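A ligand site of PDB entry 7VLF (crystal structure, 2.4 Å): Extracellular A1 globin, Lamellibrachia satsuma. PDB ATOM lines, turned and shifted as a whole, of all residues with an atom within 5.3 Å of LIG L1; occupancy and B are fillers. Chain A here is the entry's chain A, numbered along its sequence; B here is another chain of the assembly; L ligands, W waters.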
ATOM      1  N   TRP A  32      25.436  20.841  13.353  1.00  0.00           N
ATOM      2  CA  TRP A  32      25.648  22.142  13.964  1.00  0.00           C
ATOM      3  C   TRP A  32      25.683  22.060  15.491  1.00  0.00           C
ATOM      4  O   TRP A  32      26.326  22.886  16.143  1.00  0.00           O
ATOM      5  CB  TRP A  32      24.580  23.130  13.502  1.00  0.00           C
ATOM      6  CG  TRP A  32      24.743  23.528  12.078  1.00  0.00           C
ATOM      7  CD1 TRP A  32      24.243  22.903  10.981  1.00  0.00           C
ATOM      8  CD2 TRP A  32      25.478  24.658  11.588  1.00  0.00           C
ATOM      9  NE1 TRP A  32      24.611  23.560   9.838  1.00  0.00           N
ATOM     10  CE2 TRP A  32      25.381  24.646  10.181  1.00  0.00           C
ATOM     11  CE3 TRP A  32      26.220  25.679  12.206  1.00  0.00           C
ATOM     12  CZ2 TRP A  32      25.973  25.619   9.381  1.00  0.00           C
ATOM     13  CZ3 TRP A  32      26.820  26.634  11.407  1.00  0.00           C
ATOM     14  CH2 TRP A  32      26.690  26.597  10.007  1.00  0.00           C
ATOM     15  N   LEU A  45      28.695  33.878  15.780  1.00  0.00           N
ATOM     16  CA  LEU A  45      28.929  34.370  14.438  1.00  0.00           C
ATOM     17  C   LEU A  45      27.696  34.272  13.565  1.00  0.00           C
ATOM     18  O   LEU A  45      27.733  34.670  12.396  1.00  0.00           O
ATOM     19  CB  LEU A  45      30.096  33.602  13.779  1.00  0.00           C
ATOM     20  CG  LEU A  45      30.837  34.316  12.644  1.00  0.00           C
ATOM     21  CD1 LEU A  45      31.629  35.494  13.175  1.00  0.00           C
ATOM     22  CD2 LEU A  45      31.748  33.350  11.913  1.00  0.00           C
ATOM     23  N   PHE A  46      26.594  33.752  14.102  1.00  0.00           N
ATOM     24  CA  PHE A  46      25.362  33.546  13.365  1.00  0.00           C
ATOM     25  C   PHE A  46      24.198  34.240  14.044  1.00  0.00           C
ATOM     26  O   PHE A  46      23.073  33.740  14.053  1.00  0.00           O
ATOM     27  CB  PHE A  46      25.074  32.063  13.189  1.00  0.00           C
ATOM     28  CG  PHE A  46      26.151  31.304  12.466  1.00  0.00           C
ATOM     29  CD1 PHE A  46      26.176  31.250  11.093  1.00  0.00           C
ATOM     30  CD2 PHE A  46      27.138  30.641  13.177  1.00  0.00           C
ATOM     31  CE1 PHE A  46      27.166  30.556  10.421  1.00  0.00           C
ATOM     32  CE2 PHE A  46      28.129  29.948  12.515  1.00  0.00           C
ATOM     33  CZ  PHE A  46      28.150  29.903  11.141  1.00  0.00           C
ATOM     34  N   SER A  48      22.761  36.664  12.914  1.00  0.00           N
ATOM     35  CA  SER A  48      21.892  37.071  11.819  1.00  0.00           C
ATOM     36  C   SER A  48      20.872  36.013  11.435  1.00  0.00           C
ATOM     37  O   SER A  48      19.917  36.315  10.707  1.00  0.00           O
ATOM     38  CB  SER A  48      22.732  37.448  10.597  1.00  0.00           C
ATOM     39  OG  SER A  48      23.593  36.392  10.216  1.00  0.00           O
ATOM     40  N   VAL A  49      21.040  34.766  11.895  1.00  0.00           N
ATOM     41  CA  VAL A  49      20.091  33.704  11.606  1.00  0.00           C
ATOM     42  C   VAL A  49      19.364  33.261  12.877  1.00  0.00           C
ATOM     43  O   VAL A  49      18.825  32.159  12.929  1.00  0.00           O
ATOM     44  CB  VAL A  49      20.777  32.511  10.916  1.00  0.00           C
ATOM     45  CG1 VAL A  49      21.484  32.977   9.644  1.00  0.00           C
ATOM     46  CG2 VAL A  49      21.752  31.829  11.853  1.00  0.00           C
ATOM     47  N   HIS A  62      18.868  28.335   8.032  1.00  0.00           N
ATOM     48  CA  HIS A  62      20.301  28.405   7.816  1.00  0.00           C
ATOM     49  C   HIS A  62      20.920  27.015   7.725  1.00  0.00           C
ATOM     50  O   HIS A  62      21.781  26.763   6.876  1.00  0.00           O
ATOM     51  CB  HIS A  62      20.958  29.213   8.946  1.00  0.00           C
ATOM     52  CG  HIS A  62      22.451  29.266   8.858  1.00  0.00           C
ATOM     53  ND1 HIS A  62      23.115  29.706   7.745  1.00  0.00           N
ATOM     54  CD2 HIS A  62      23.406  28.924   9.764  1.00  0.00           C
ATOM     55  CE1 HIS A  62      24.425  29.648   7.953  1.00  0.00           C
ATOM     56  NE2 HIS A  62      24.627  29.174   9.170  1.00  0.00           N
ATOM     57  N   ARG A  65      20.081  25.565   4.205  1.00  0.00           N
ATOM     58  CA  ARG A  65      20.827  26.117   3.080  1.00  0.00           C
ATOM     59  C   ARG A  65      22.276  25.643   3.095  1.00  0.00           C
ATOM     60  O   ARG A  65      22.852  25.389   2.030  1.00  0.00           O
ATOM     61  CB  ARG A  65      20.762  27.649   3.100  1.00  0.00           C
ATOM     62  CG  ARG A  65      19.434  28.213   2.616  1.00  0.00           C
ATOM     63  CD  ARG A  65      19.489  29.733   2.516  1.00  0.00           C
ATOM     64  NE  ARG A  65      19.745  30.355   3.808  1.00  0.00           N
ATOM     65  CZ  ARG A  65      18.798  30.774   4.634  1.00  0.00           C
ATOM     66  NH1 ARG A  65      17.515  30.624   4.299  1.00  0.00           N
ATOM     67  NH2 ARG A  65      19.115  31.334   5.787  1.00  0.00           N
ATOM     68  N   VAL A  66      22.872  25.518   4.280  1.00  0.00           N
ATOM     69  CA  VAL A  66      24.283  25.131   4.358  1.00  0.00           C
ATOM     70  C   VAL A  66      24.469  23.683   3.931  1.00  0.00           C
ATOM     71  O   VAL A  66      25.239  23.385   3.005  1.00  0.00           O
ATOM     72  CB  VAL A  66      24.830  25.377   5.773  1.00  0.00           C
ATOM     73  CG1 VAL A  66      26.182  24.719   5.933  1.00  0.00           C
ATOM     74  CG2 VAL A  66      24.933  26.863   6.047  1.00  0.00           C
ATOM     75  N   GLY A  69      23.683  23.115   0.301  1.00  0.00           N
ATOM     76  CA  GLY A  69      24.802  23.427  -0.575  1.00  0.00           C
ATOM     77  C   GLY A  69      25.902  22.387  -0.484  1.00  0.00           C
ATOM     78  O   GLY A  69      26.556  22.075  -1.488  1.00  0.00           O
ATOM     79  N   LEU A  70      26.129  21.846   0.709  1.00  0.00           N
ATOM     80  CA  LEU A  70      27.068  20.739   0.855  1.00  0.00           C
ATOM     81  C   LEU A  70      26.585  19.523   0.076  1.00  0.00           C
ATOM     82  O   LEU A  70      27.387  18.785  -0.512  1.00  0.00           O
ATOM     83  CB  LEU A  70      27.264  20.395   2.329  1.00  0.00           C
ATOM     84  CG  LEU A  70      28.279  19.305   2.658  1.00  0.00           C
ATOM     85  CD1 LEU A  70      29.608  19.607   1.986  1.00  0.00           C
ATOM     86  CD2 LEU A  70      28.460  19.154   4.159  1.00  0.00           C
ATOM     87  N   ARG A  72      24.811  19.710  -2.697  1.00  0.00           N
ATOM     88  CA  ARG A  72      24.987  20.005  -4.109  1.00  0.00           C
ATOM     89  C   ARG A  72      26.455  20.030  -4.515  1.00  0.00           C
ATOM     90  O   ARG A  72      26.782  19.735  -5.663  1.00  0.00           O
ATOM     91  CB  ARG A  72      24.316  21.334  -4.461  1.00  0.00           C
ATOM     92  CG  ARG A  72      25.152  22.581  -4.246  1.00  0.00           C
ATOM     93  CD  ARG A  72      24.448  23.812  -4.804  1.00  0.00           C
ATOM     94  NE  ARG A  72      25.320  24.986  -4.847  1.00  0.00           N
ATOM     95  CZ  ARG A  72      25.273  25.985  -3.979  1.00  0.00           C
ATOM     96  NH1 ARG A  72      24.383  25.972  -2.992  1.00  0.00           N
ATOM     97  NH2 ARG A  72      26.099  27.013  -4.090  1.00  0.00           N
ATOM     98  N   VAL A  73      27.350  20.346  -3.577  1.00  0.00           N
ATOM     99  CA  VAL A  73      28.774  20.284  -3.867  1.00  0.00           C
ATOM    100  C   VAL A  73      29.231  18.831  -3.975  1.00  0.00           C
ATOM    101  O   VAL A  73      29.976  18.469  -4.880  1.00  0.00           O
ATOM    102  CB  VAL A  73      29.576  21.063  -2.808  1.00  0.00           C
ATOM    103  CG1 VAL A  73      31.047  20.712  -2.882  1.00  0.00           C
ATOM    104  CG2 VAL A  73      29.370  22.548  -2.981  1.00  0.00           C
ATOM    105  N   LEU A  90      30.767  29.966  -3.984  1.00  0.00           N
ATOM    106  CA  LEU A  90      30.688  29.970  -2.528  1.00  0.00           C
ATOM    107  C   LEU A  90      31.826  30.763  -1.899  1.00  0.00           C
ATOM    108  O   LEU A  90      31.657  31.352  -0.824  1.00  0.00           O
ATOM    109  CB  LEU A  90      30.684  28.532  -2.007  1.00  0.00           C
ATOM    110  CG  LEU A  90      29.516  27.665  -2.463  1.00  0.00           C
ATOM    111  CD1 LEU A  90      29.815  26.195  -2.210  1.00  0.00           C
ATOM    112  CD2 LEU A  90      28.230  28.067  -1.745  1.00  0.00           C
ATOM    113  N   GLN A  93      31.030  34.360  -1.914  1.00  0.00           N
ATOM    114  CA  GLN A  93      29.960  34.626  -0.956  1.00  0.00           C
ATOM    115  C   GLN A  93      30.469  34.638   0.483  1.00  0.00           C
ATOM    116  O   GLN A  93      30.005  35.435   1.295  1.00  0.00           O
ATOM    117  CB  GLN A  93      28.833  33.597  -1.090  1.00  0.00           C
ATOM    118  CG  GLN A  93      28.015  33.726  -2.356  1.00  0.00           C
ATOM    119  CD  GLN A  93      26.921  32.682  -2.461  1.00  0.00           C
ATOM    120  OE1 GLN A  93      27.115  31.527  -2.077  1.00  0.00           O
ATOM    121  NE2 GLN A  93      25.769  33.078  -2.991  1.00  0.00           N
ATOM    122  N   HIS A  94      31.419  33.749   0.812  1.00  0.00           N
ATOM    123  CA  HIS A  94      31.942  33.672   2.160  1.00  0.00           C
ATOM    124  C   HIS A  94      33.089  34.643   2.411  1.00  0.00           C
ATOM    125  O   HIS A  94      33.237  35.147   3.527  1.00  0.00           O
ATOM    126  CB  HIS A  94      32.397  32.244   2.474  1.00  0.00           C
ATOM    127  CG  HIS A  94      31.294  31.343   2.938  1.00  0.00           C
ATOM    128  ND1 HIS A  94      30.444  30.692   2.070  1.00  0.00           N
ATOM    129  CD2 HIS A  94      30.898  30.991   4.186  1.00  0.00           C
ATOM    130  CE1 HIS A  94      29.581  29.972   2.752  1.00  0.00           C
ATOM    131  NE2 HIS A  94      29.825  30.139   4.044  1.00  0.00           N
ATOM    132  N   ARG A  97      32.410  37.927   4.248  1.00  0.00           N
ATOM    133  CA  ARG A  97      32.265  37.824   5.693  1.00  0.00           C
ATOM    134  C   ARG A  97      33.609  37.836   6.394  1.00  0.00           C
ATOM    135  O   ARG A  97      33.698  38.240   7.559  1.00  0.00           O
ATOM    136  CB  ARG A  97      31.467  36.568   6.063  1.00  0.00           C
ATOM    137  CG  ARG A  97      30.018  36.610   5.618  1.00  0.00           C
ATOM    138  CD  ARG A  97      29.582  35.278   5.042  1.00  0.00           C
ATOM    139  NE  ARG A  97      28.217  35.328   4.517  1.00  0.00           N
ATOM    140  CZ  ARG A  97      27.690  34.408   3.714  1.00  0.00           C
ATOM    141  NH1 ARG A  97      28.406  33.374   3.314  1.00  0.00           N
ATOM    142  NH2 ARG A  97      26.443  34.552   3.287  1.00  0.00           N
ATOM    143  N   LEU A  99      35.713  35.176   7.339  1.00  0.00           N
ATOM    144  CA  LEU A  99      35.620  34.255   8.460  1.00  0.00           C
ATOM    145  C   LEU A  99      36.961  33.592   8.743  1.00  0.00           C
ATOM    146  O   LEU A  99      37.832  33.486   7.874  1.00  0.00           O
ATOM    147  CB  LEU A  99      34.573  33.174   8.193  1.00  0.00           C
ATOM    148  CG  LEU A  99      33.245  33.615   7.573  1.00  0.00           C
ATOM    149  CD1 LEU A  99      33.247  33.343   6.079  1.00  0.00           C
ATOM    150  CD2 LEU A  99      32.085  32.916   8.240  1.00  0.00           C
ATOM    151  N   ASN A 103      37.360  27.479  11.391  1.00  0.00           N
ATOM    152  CA  ASN A 103      35.994  26.985  11.564  1.00  0.00           C
ATOM    153  C   ASN A 103      35.659  25.922  10.529  1.00  0.00           C
ATOM    154  O   ASN A 103      34.925  24.974  10.823  1.00  0.00           O
ATOM    155  CB  ASN A 103      35.009  28.142  11.478  1.00  0.00           C
ATOM    156  CG  ASN A 103      35.315  29.254  12.459  1.00  0.00           C
ATOM    157  OD1 ASN A 103      35.521  30.398  12.069  1.00  0.00           O
ATOM    158  ND2 ASN A 103      35.358  28.912  13.735  1.00  0.00           N
ATOM    159  N   PHE A 104      36.185  26.060   9.306  1.00  0.00           N
ATOM    160  CA  PHE A 104      36.007  25.005   8.315  1.00  0.00           C
ATOM    161  C   PHE A 104      36.700  23.726   8.740  1.00  0.00           C
ATOM    162  O   PHE A 104      36.288  22.628   8.333  1.00  0.00           O
ATOM    163  CB  PHE A 104      36.530  25.481   6.948  1.00  0.00           C
ATOM    164  CG  PHE A 104      35.643  26.488   6.284  1.00  0.00           C
ATOM    165  CD1 PHE A 104      35.604  27.806   6.735  1.00  0.00           C
ATOM    166  CD2 PHE A 104      34.850  26.141   5.209  1.00  0.00           C
ATOM    167  CE1 PHE A 104      34.788  28.740   6.114  1.00  0.00           C
ATOM    168  CE2 PHE A 104      34.039  27.065   4.589  1.00  0.00           C
ATOM    169  CZ  PHE A 104      34.008  28.365   5.042  1.00  0.00           C
ATOM    170  N   PHE A 107      34.210  22.458  11.054  1.00  0.00           N
ATOM    171  CA  PHE A 107      33.080  22.016  10.247  1.00  0.00           C
ATOM    172  C   PHE A 107      33.269  20.578   9.787  1.00  0.00           C
ATOM    173  O   PHE A 107      32.358  19.741   9.881  1.00  0.00           O
ATOM    174  CB  PHE A 107      32.894  22.950   9.060  1.00  0.00           C
ATOM    175  CG  PHE A 107      31.696  22.628   8.212  1.00  0.00           C
ATOM    176  CD1 PHE A 107      30.460  23.189   8.480  1.00  0.00           C
ATOM    177  CD2 PHE A 107      31.799  21.756   7.131  1.00  0.00           C
ATOM    178  CE1 PHE A 107      29.360  22.896   7.711  1.00  0.00           C
ATOM    179  CE2 PHE A 107      30.693  21.449   6.354  1.00  0.00           C
ATOM    180  CZ  PHE A 107      29.479  22.021   6.648  1.00  0.00           C
ATOM    181  N   TYR A 132      37.172  16.460   1.716  1.00  0.00           N
ATOM    182  CA  TYR A 132      36.722  17.677   2.361  1.00  0.00           C
ATOM    183  C   TYR A 132      37.722  18.808   2.170  1.00  0.00           C
ATOM    184  O   TYR A 132      37.330  19.981   2.126  1.00  0.00           O
ATOM    185  CB  TYR A 132      36.484  17.449   3.851  1.00  0.00           C
ATOM    186  CG  TYR A 132      36.076  18.704   4.588  1.00  0.00           C
ATOM    187  CD1 TYR A 132      34.785  19.206   4.463  1.00  0.00           C
ATOM    188  CD2 TYR A 132      36.971  19.381   5.388  1.00  0.00           C
ATOM    189  CE1 TYR A 132      34.409  20.360   5.129  1.00  0.00           C
ATOM    190  CE2 TYR A 132      36.609  20.531   6.063  1.00  0.00           C
ATOM    191  CZ  TYR A 132      35.325  21.013   5.930  1.00  0.00           C
ATOM    192  OH  TYR A 132      34.954  22.158   6.597  1.00  0.00           O
ATOM    193  N   ILE A 135      36.832  20.799  -0.799  1.00  0.00           N
ATOM    194  CA  ILE A 135      35.719  21.716  -0.600  1.00  0.00           C
ATOM    195  C   ILE A 135      36.182  22.963   0.137  1.00  0.00           C
ATOM    196  O   ILE A 135      35.925  24.095  -0.299  1.00  0.00           O
ATOM    197  CB  ILE A 135      34.576  21.009   0.148  1.00  0.00           C
ATOM    198  CG1 ILE A 135      34.006  19.869  -0.694  1.00  0.00           C
ATOM    199  CG2 ILE A 135      33.486  22.006   0.517  1.00  0.00           C
ATOM    200  CD1 ILE A 135      32.881  19.121  -0.014  1.00  0.00           C
ATOM    201  N   ILE A 139      36.341  27.027  -1.033  1.00  0.00           N
ATOM    202  CA  ILE A 139      35.552  28.083  -0.396  1.00  0.00           C
ATOM    203  C   ILE A 139      36.491  29.076   0.288  1.00  0.00           C
ATOM    204  O   ILE A 139      36.448  30.272  -0.005  1.00  0.00           O
ATOM    205  CB  ILE A 139      34.555  27.486   0.617  1.00  0.00           C
ATOM    206  CG1 ILE A 139      33.598  26.526  -0.090  1.00  0.00           C
ATOM    207  CG2 ILE A 139      33.774  28.593   1.307  1.00  0.00           C
ATOM    208  CD1 ILE A 139      32.617  25.863   0.839  1.00  0.00           C
ATOM    209  N   HIS B  94      13.444  33.908   2.164  1.00  0.00           N
ATOM    210  CA  HIS B  94      14.827  34.246   1.877  1.00  0.00           C
ATOM    211  C   HIS B  94      15.147  34.160   0.399  1.00  0.00           C
ATOM    212  O   HIS B  94      15.965  34.941  -0.104  1.00  0.00           O
ATOM    213  CB  HIS B  94      15.768  33.339   2.675  1.00  0.00           C
ATOM    214  CG  HIS B  94      17.152  33.882   2.838  1.00  0.00           C
ATOM    215  ND1 HIS B  94      18.144  33.704   1.906  1.00  0.00           N
ATOM    216  CD2 HIS B  94      17.700  34.620   3.845  1.00  0.00           C
ATOM    217  CE1 HIS B  94      19.248  34.297   2.322  1.00  0.00           C
ATOM    218  NE2 HIS B  94      19.005  34.861   3.487  1.00  0.00           N
ATOM    219  N   GLN B  98      16.220  37.402  -2.523  1.00  0.00           N
ATOM    220  CA  GLN B  98      17.327  37.306  -3.477  1.00  0.00           C
ATOM    221  C   GLN B  98      16.863  37.579  -4.896  1.00  0.00           C
ATOM    222  O   GLN B  98      17.578  38.224  -5.675  1.00  0.00           O
ATOM    223  CB  GLN B  98      17.973  35.922  -3.379  1.00  0.00           C
ATOM    224  CG  GLN B  98      18.541  35.591  -2.012  1.00  0.00           C
ATOM    225  CD  GLN B  98      19.088  34.172  -1.941  1.00  0.00           C
ATOM    226  OE1 GLN B  98      19.050  33.432  -2.925  1.00  0.00           O
ATOM    227  NE2 GLN B  98      19.610  33.803  -0.778  1.00  0.00           N
HETATM  228  C1  LIG L   1      25.887  31.334   4.607  1.00  0.00           C
HETATM  229  C2  LIG L   1      27.198  27.135   2.525  1.00  0.00           C
HETATM  230  C3  LIG L   1      30.585  26.490   5.923  1.00  0.00           C
HETATM  231  C4  LIG L   1      29.438  30.747   7.952  1.00  0.00           C
HETATM  232  C5  LIG L   1      25.895  30.213   3.790  1.00  0.00           C
HETATM  233  C6  LIG L   1      24.925  29.889   2.769  1.00  0.00           C
HETATM  234  C7  LIG L   1      25.286  28.727   2.207  1.00  0.00           C
HETATM  235  C8  LIG L   1      26.508  28.283   2.837  1.00  0.00           C
HETATM  236  C9  LIG L   1      24.563  27.966   1.068  1.00  0.00           C
HETATM  237  C10 LIG L   1      23.667  30.750   2.433  1.00  0.00           C
HETATM  238  C11 LIG L   1      23.702  31.288   1.003  1.00  0.00           C
HETATM  239  C12 LIG L   1      22.501  32.148   0.752  1.00  0.00           C
HETATM  240  O1  LIG L   1      22.058  32.847   1.706  1.00  0.00           O
HETATM  241  O2  LIG L   1      21.978  32.145  -0.393  1.00  0.00           O
HETATM  242  C13 LIG L   1      28.239  26.607   3.245  1.00  0.00           C
HETATM  243  C14 LIG L   1      28.970  25.391   2.938  1.00  0.00           C
HETATM  244  C15 LIG L   1      29.906  25.209   3.885  1.00  0.00           C
HETATM  245  C16 LIG L   1      29.790  26.314   4.816  1.00  0.00           C
HETATM  246  C17 LIG L   1      28.664  24.499   1.705  1.00  0.00           C
HETATM  247  C18 LIG L   1      30.965  24.092   4.061  1.00  0.00           C
HETATM  248  C19 LIG L   1      31.175  23.079   3.210  1.00  0.00           C
HETATM  249  C20 LIG L   1      30.580  27.582   6.755  1.00  0.00           C
HETATM  250  C21 LIG L   1      31.484  27.784   7.858  1.00  0.00           C
HETATM  251  C22 LIG L   1      31.181  28.941   8.436  1.00  0.00           C
HETATM  252  C23 LIG L   1      30.067  29.534   7.705  1.00  0.00           C
HETATM  253  C24 LIG L   1      32.597  26.815   8.314  1.00  0.00           C
HETATM  254  C25 LIG L   1      31.957  29.481   9.659  1.00  0.00           C
HETATM  255  C26 LIG L   1      31.410  30.354  10.500  1.00  0.00           C
HETATM  256  C27 LIG L   1      28.371  31.300   7.273  1.00  0.00           C
HETATM  257  C28 LIG L   1      27.711  32.540   7.610  1.00  0.00           C
HETATM  258  C29 LIG L   1      26.604  32.725   6.567  1.00  0.00           C
HETATM  259  C30 LIG L   1      26.697  31.570   5.695  1.00  0.00           C
HETATM  260  C31 LIG L   1      28.047  33.494   8.781  1.00  0.00           C
HETATM  261  C32 LIG L   1      25.613  33.903   6.498  1.00  0.00           C
HETATM  262  C33 LIG L   1      24.188  33.404   6.779  1.00  0.00           C
HETATM  263  C34 LIG L   1      23.229  34.559   6.792  1.00  0.00           C
HETATM  264  O3  LIG L   1      23.442  35.534   7.567  1.00  0.00           O
HETATM  265  O4  LIG L   1      22.216  34.503   6.034  1.00  0.00           O
HETATM  266  N1  LIG L   1      26.856  29.213   3.798  1.00  0.00           N
HETATM  267  N2  LIG L   1      28.775  27.144   4.400  1.00  0.00           N
HETATM  268  N3  LIG L   1      29.727  28.667   6.685  1.00  0.00           N
HETATM  269  N4  LIG L   1      27.748  30.770   6.145  1.00  0.00           N
HETATM  270 FE1  LIG L   1      28.325  29.023   5.192  1.00  0.00          FE
HETATM  271  C1  LG2 L   2      19.759  32.401  -8.541  1.00  0.00           C
HETATM  272  C2  LG2 L   2      16.478  29.254  -6.860  1.00  0.00           C
HETATM  273  C3  LG2 L   2      13.573  30.291 -10.607  1.00  0.00           C
HETATM  274  C4  LG2 L   2      16.568  33.855 -11.971  1.00  0.00           C
HETATM  275  C5  LG2 L   2      19.154  31.404  -7.818  1.00  0.00           C
HETATM  276  C6  LG2 L   2      19.788  30.636  -6.765  1.00  0.00           C
HETATM  277  C7  LG2 L   2      18.881  29.769  -6.294  1.00  0.00           C
HETATM  278  C8  LG2 L   2      17.653  29.960  -7.032  1.00  0.00           C
HETATM  279  C9  LG2 L   2      19.119  28.743  -5.170  1.00  0.00           C
HETATM  280  C10 LG2 L   2      21.247  30.790  -6.276  1.00  0.00           C
HETATM  281  C11 LG2 L   2      21.359  31.907  -5.246  1.00  0.00           C
HETATM  282  C12 LG2 L   2      22.805  32.099  -4.882  1.00  0.00           C
HETATM  283  O1  LG2 L   2      23.645  32.249  -5.811  1.00  0.00           O
HETATM  284  O2  LG2 L   2      23.115  32.112  -3.667  1.00  0.00           O
HETATM  285  C13 LG2 L   2      15.404  29.250  -7.719  1.00  0.00           C
HETATM  286  C14 LG2 L   2      14.212  28.434  -7.602  1.00  0.00           C
HETATM  287  C15 LG2 L   2      13.409  28.711  -8.635  1.00  0.00           C
HETATM  288  C16 LG2 L   2      14.070  29.724  -9.447  1.00  0.00           C
HETATM  289  C17 LG2 L   2      13.997  27.430  -6.438  1.00  0.00           C
HETATM  290  C18 LG2 L   2      12.014  28.146  -9.006  1.00  0.00           C
HETATM  291  C19 LG2 L   2      11.313  27.286  -8.241  1.00  0.00           C
HETATM  292  C20 LG2 L   2      14.121  31.354 -11.293  1.00  0.00           C
HETATM  293  C21 LG2 L   2      13.550  31.985 -12.476  1.00  0.00           C
HETATM  294  C22 LG2 L   2      14.383  32.982 -12.846  1.00  0.00           C
HETATM  295  C23 LG2 L   2      15.499  32.988 -11.920  1.00  0.00           C
HETATM  296  C24 LG2 L   2      12.215  31.544 -13.112  1.00  0.00           C
HETATM  297  C25 LG2 L   2      14.290  33.979 -14.030  1.00  0.00           C
HETATM  298  C26 LG2 L   2      13.403  33.903 -15.030  1.00  0.00           C
HETATM  299  C27 LG2 L   2      17.723  33.787 -11.211  1.00  0.00           C
HETATM  300  C28 LG2 L   2      18.892  34.610 -11.388  1.00  0.00           C
HETATM  301  C29 LG2 L   2      19.887  34.159 -10.310  1.00  0.00           C
HETATM  302  C30 LG2 L   2      19.210  33.096  -9.602  1.00  0.00           C
HETATM  303  C31 LG2 L   2      19.097  35.730 -12.434  1.00  0.00           C
HETATM  304  C32 LG2 L   2      21.305  34.693 -10.028  1.00  0.00           C
HETATM  305  C33 LG2 L   2      22.286  34.255 -11.118  1.00  0.00           C
HETATM  306  C34 LG2 L   2      23.676  34.605 -10.667  1.00  0.00           C
HETATM  307  O3  LG2 L   2      23.920  34.701  -9.437  1.00  0.00           O
HETATM  308  O4  LG2 L   2      24.558  34.799 -11.556  1.00  0.00           O
HETATM  309  N1  LG2 L   2      17.859  30.970  -7.952  1.00  0.00           N
HETATM  310  N2  LG2 L   2      15.280  30.029  -8.862  1.00  0.00           N
HETATM  311  N3  LG2 L   2      15.303  31.983 -10.991  1.00  0.00           N
HETATM  312  N4  LG2 L   2      17.955  32.906 -10.157  1.00  0.00           N
HETATM  313 FE1  LG2 L   2      16.517  31.571  -9.442  1.00  0.00          FE
HETATM  314  O   HOH W   1      19.885  35.922   7.621  1.00  0.00           O
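Residues that only touch LIG L1: His 94 of chain B (3.2 Å), Leu 45 (3.3 Å), Phe 46 (3.4 Å), Arg 97 (3.4 Å), Leu 99 (3.4 Å), Phe 107 (3.5 Å), Phe 104 (3.5 Å), Val 49 (3.7 Å), Ile 135 (3.7 Å), His 62 (3.7 Å), Val 66 (3.8 Å), Asn 103 (3.8 Å), Leu 70 (3.8 Å) and Ile 139 (3.9 Å).
Of the 25 residues printed, 18 come within 4 Å of LIG L1.
A ring nitrogen (NE2) of His 94 of chain A binds an iron atom (FE1) of LIG L1, at 2.2 Å.
The side-chain amide nitrogen (NE2) of Gln 98 of chain B is in hydrogen-bond range of an oxygen (O2) of LIG L1, 2.9 Å away.
The guanidinium group (NE) of Arg 65 is in salt-bridge range of an oxygen (O1) of LIG L1 (3.997 Å).
NE2 of Gln 93 is in hydrogen-bond range of O2 of LG2 L2.
The side-chain hydroxyl (OG) of Ser 48 sits at hydrogen-bond distance from an oxygen (O3) of LIG L1 (2.8 Å).
Water W1 lies within hydrogen-bond range of the backbone carbonyl oxygen of Ser 48 (3.1 Å) and an oxygen (O4) of LIG L1 (3.2 Å).
NE2 of Gln 98 of chain B sits at hydrogen-bond distance from ND1 of His 94 of chain B.
O of Gln 93 is in hydrogen-bond range of NH1 of Arg 97 (3.3 Å).
A ring nitrogen (ND1) of His 94 of chain A sits at hydrogen-bond distance from the backbone carbonyl oxygen (O) of Leu 90, 3.2 Å away.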
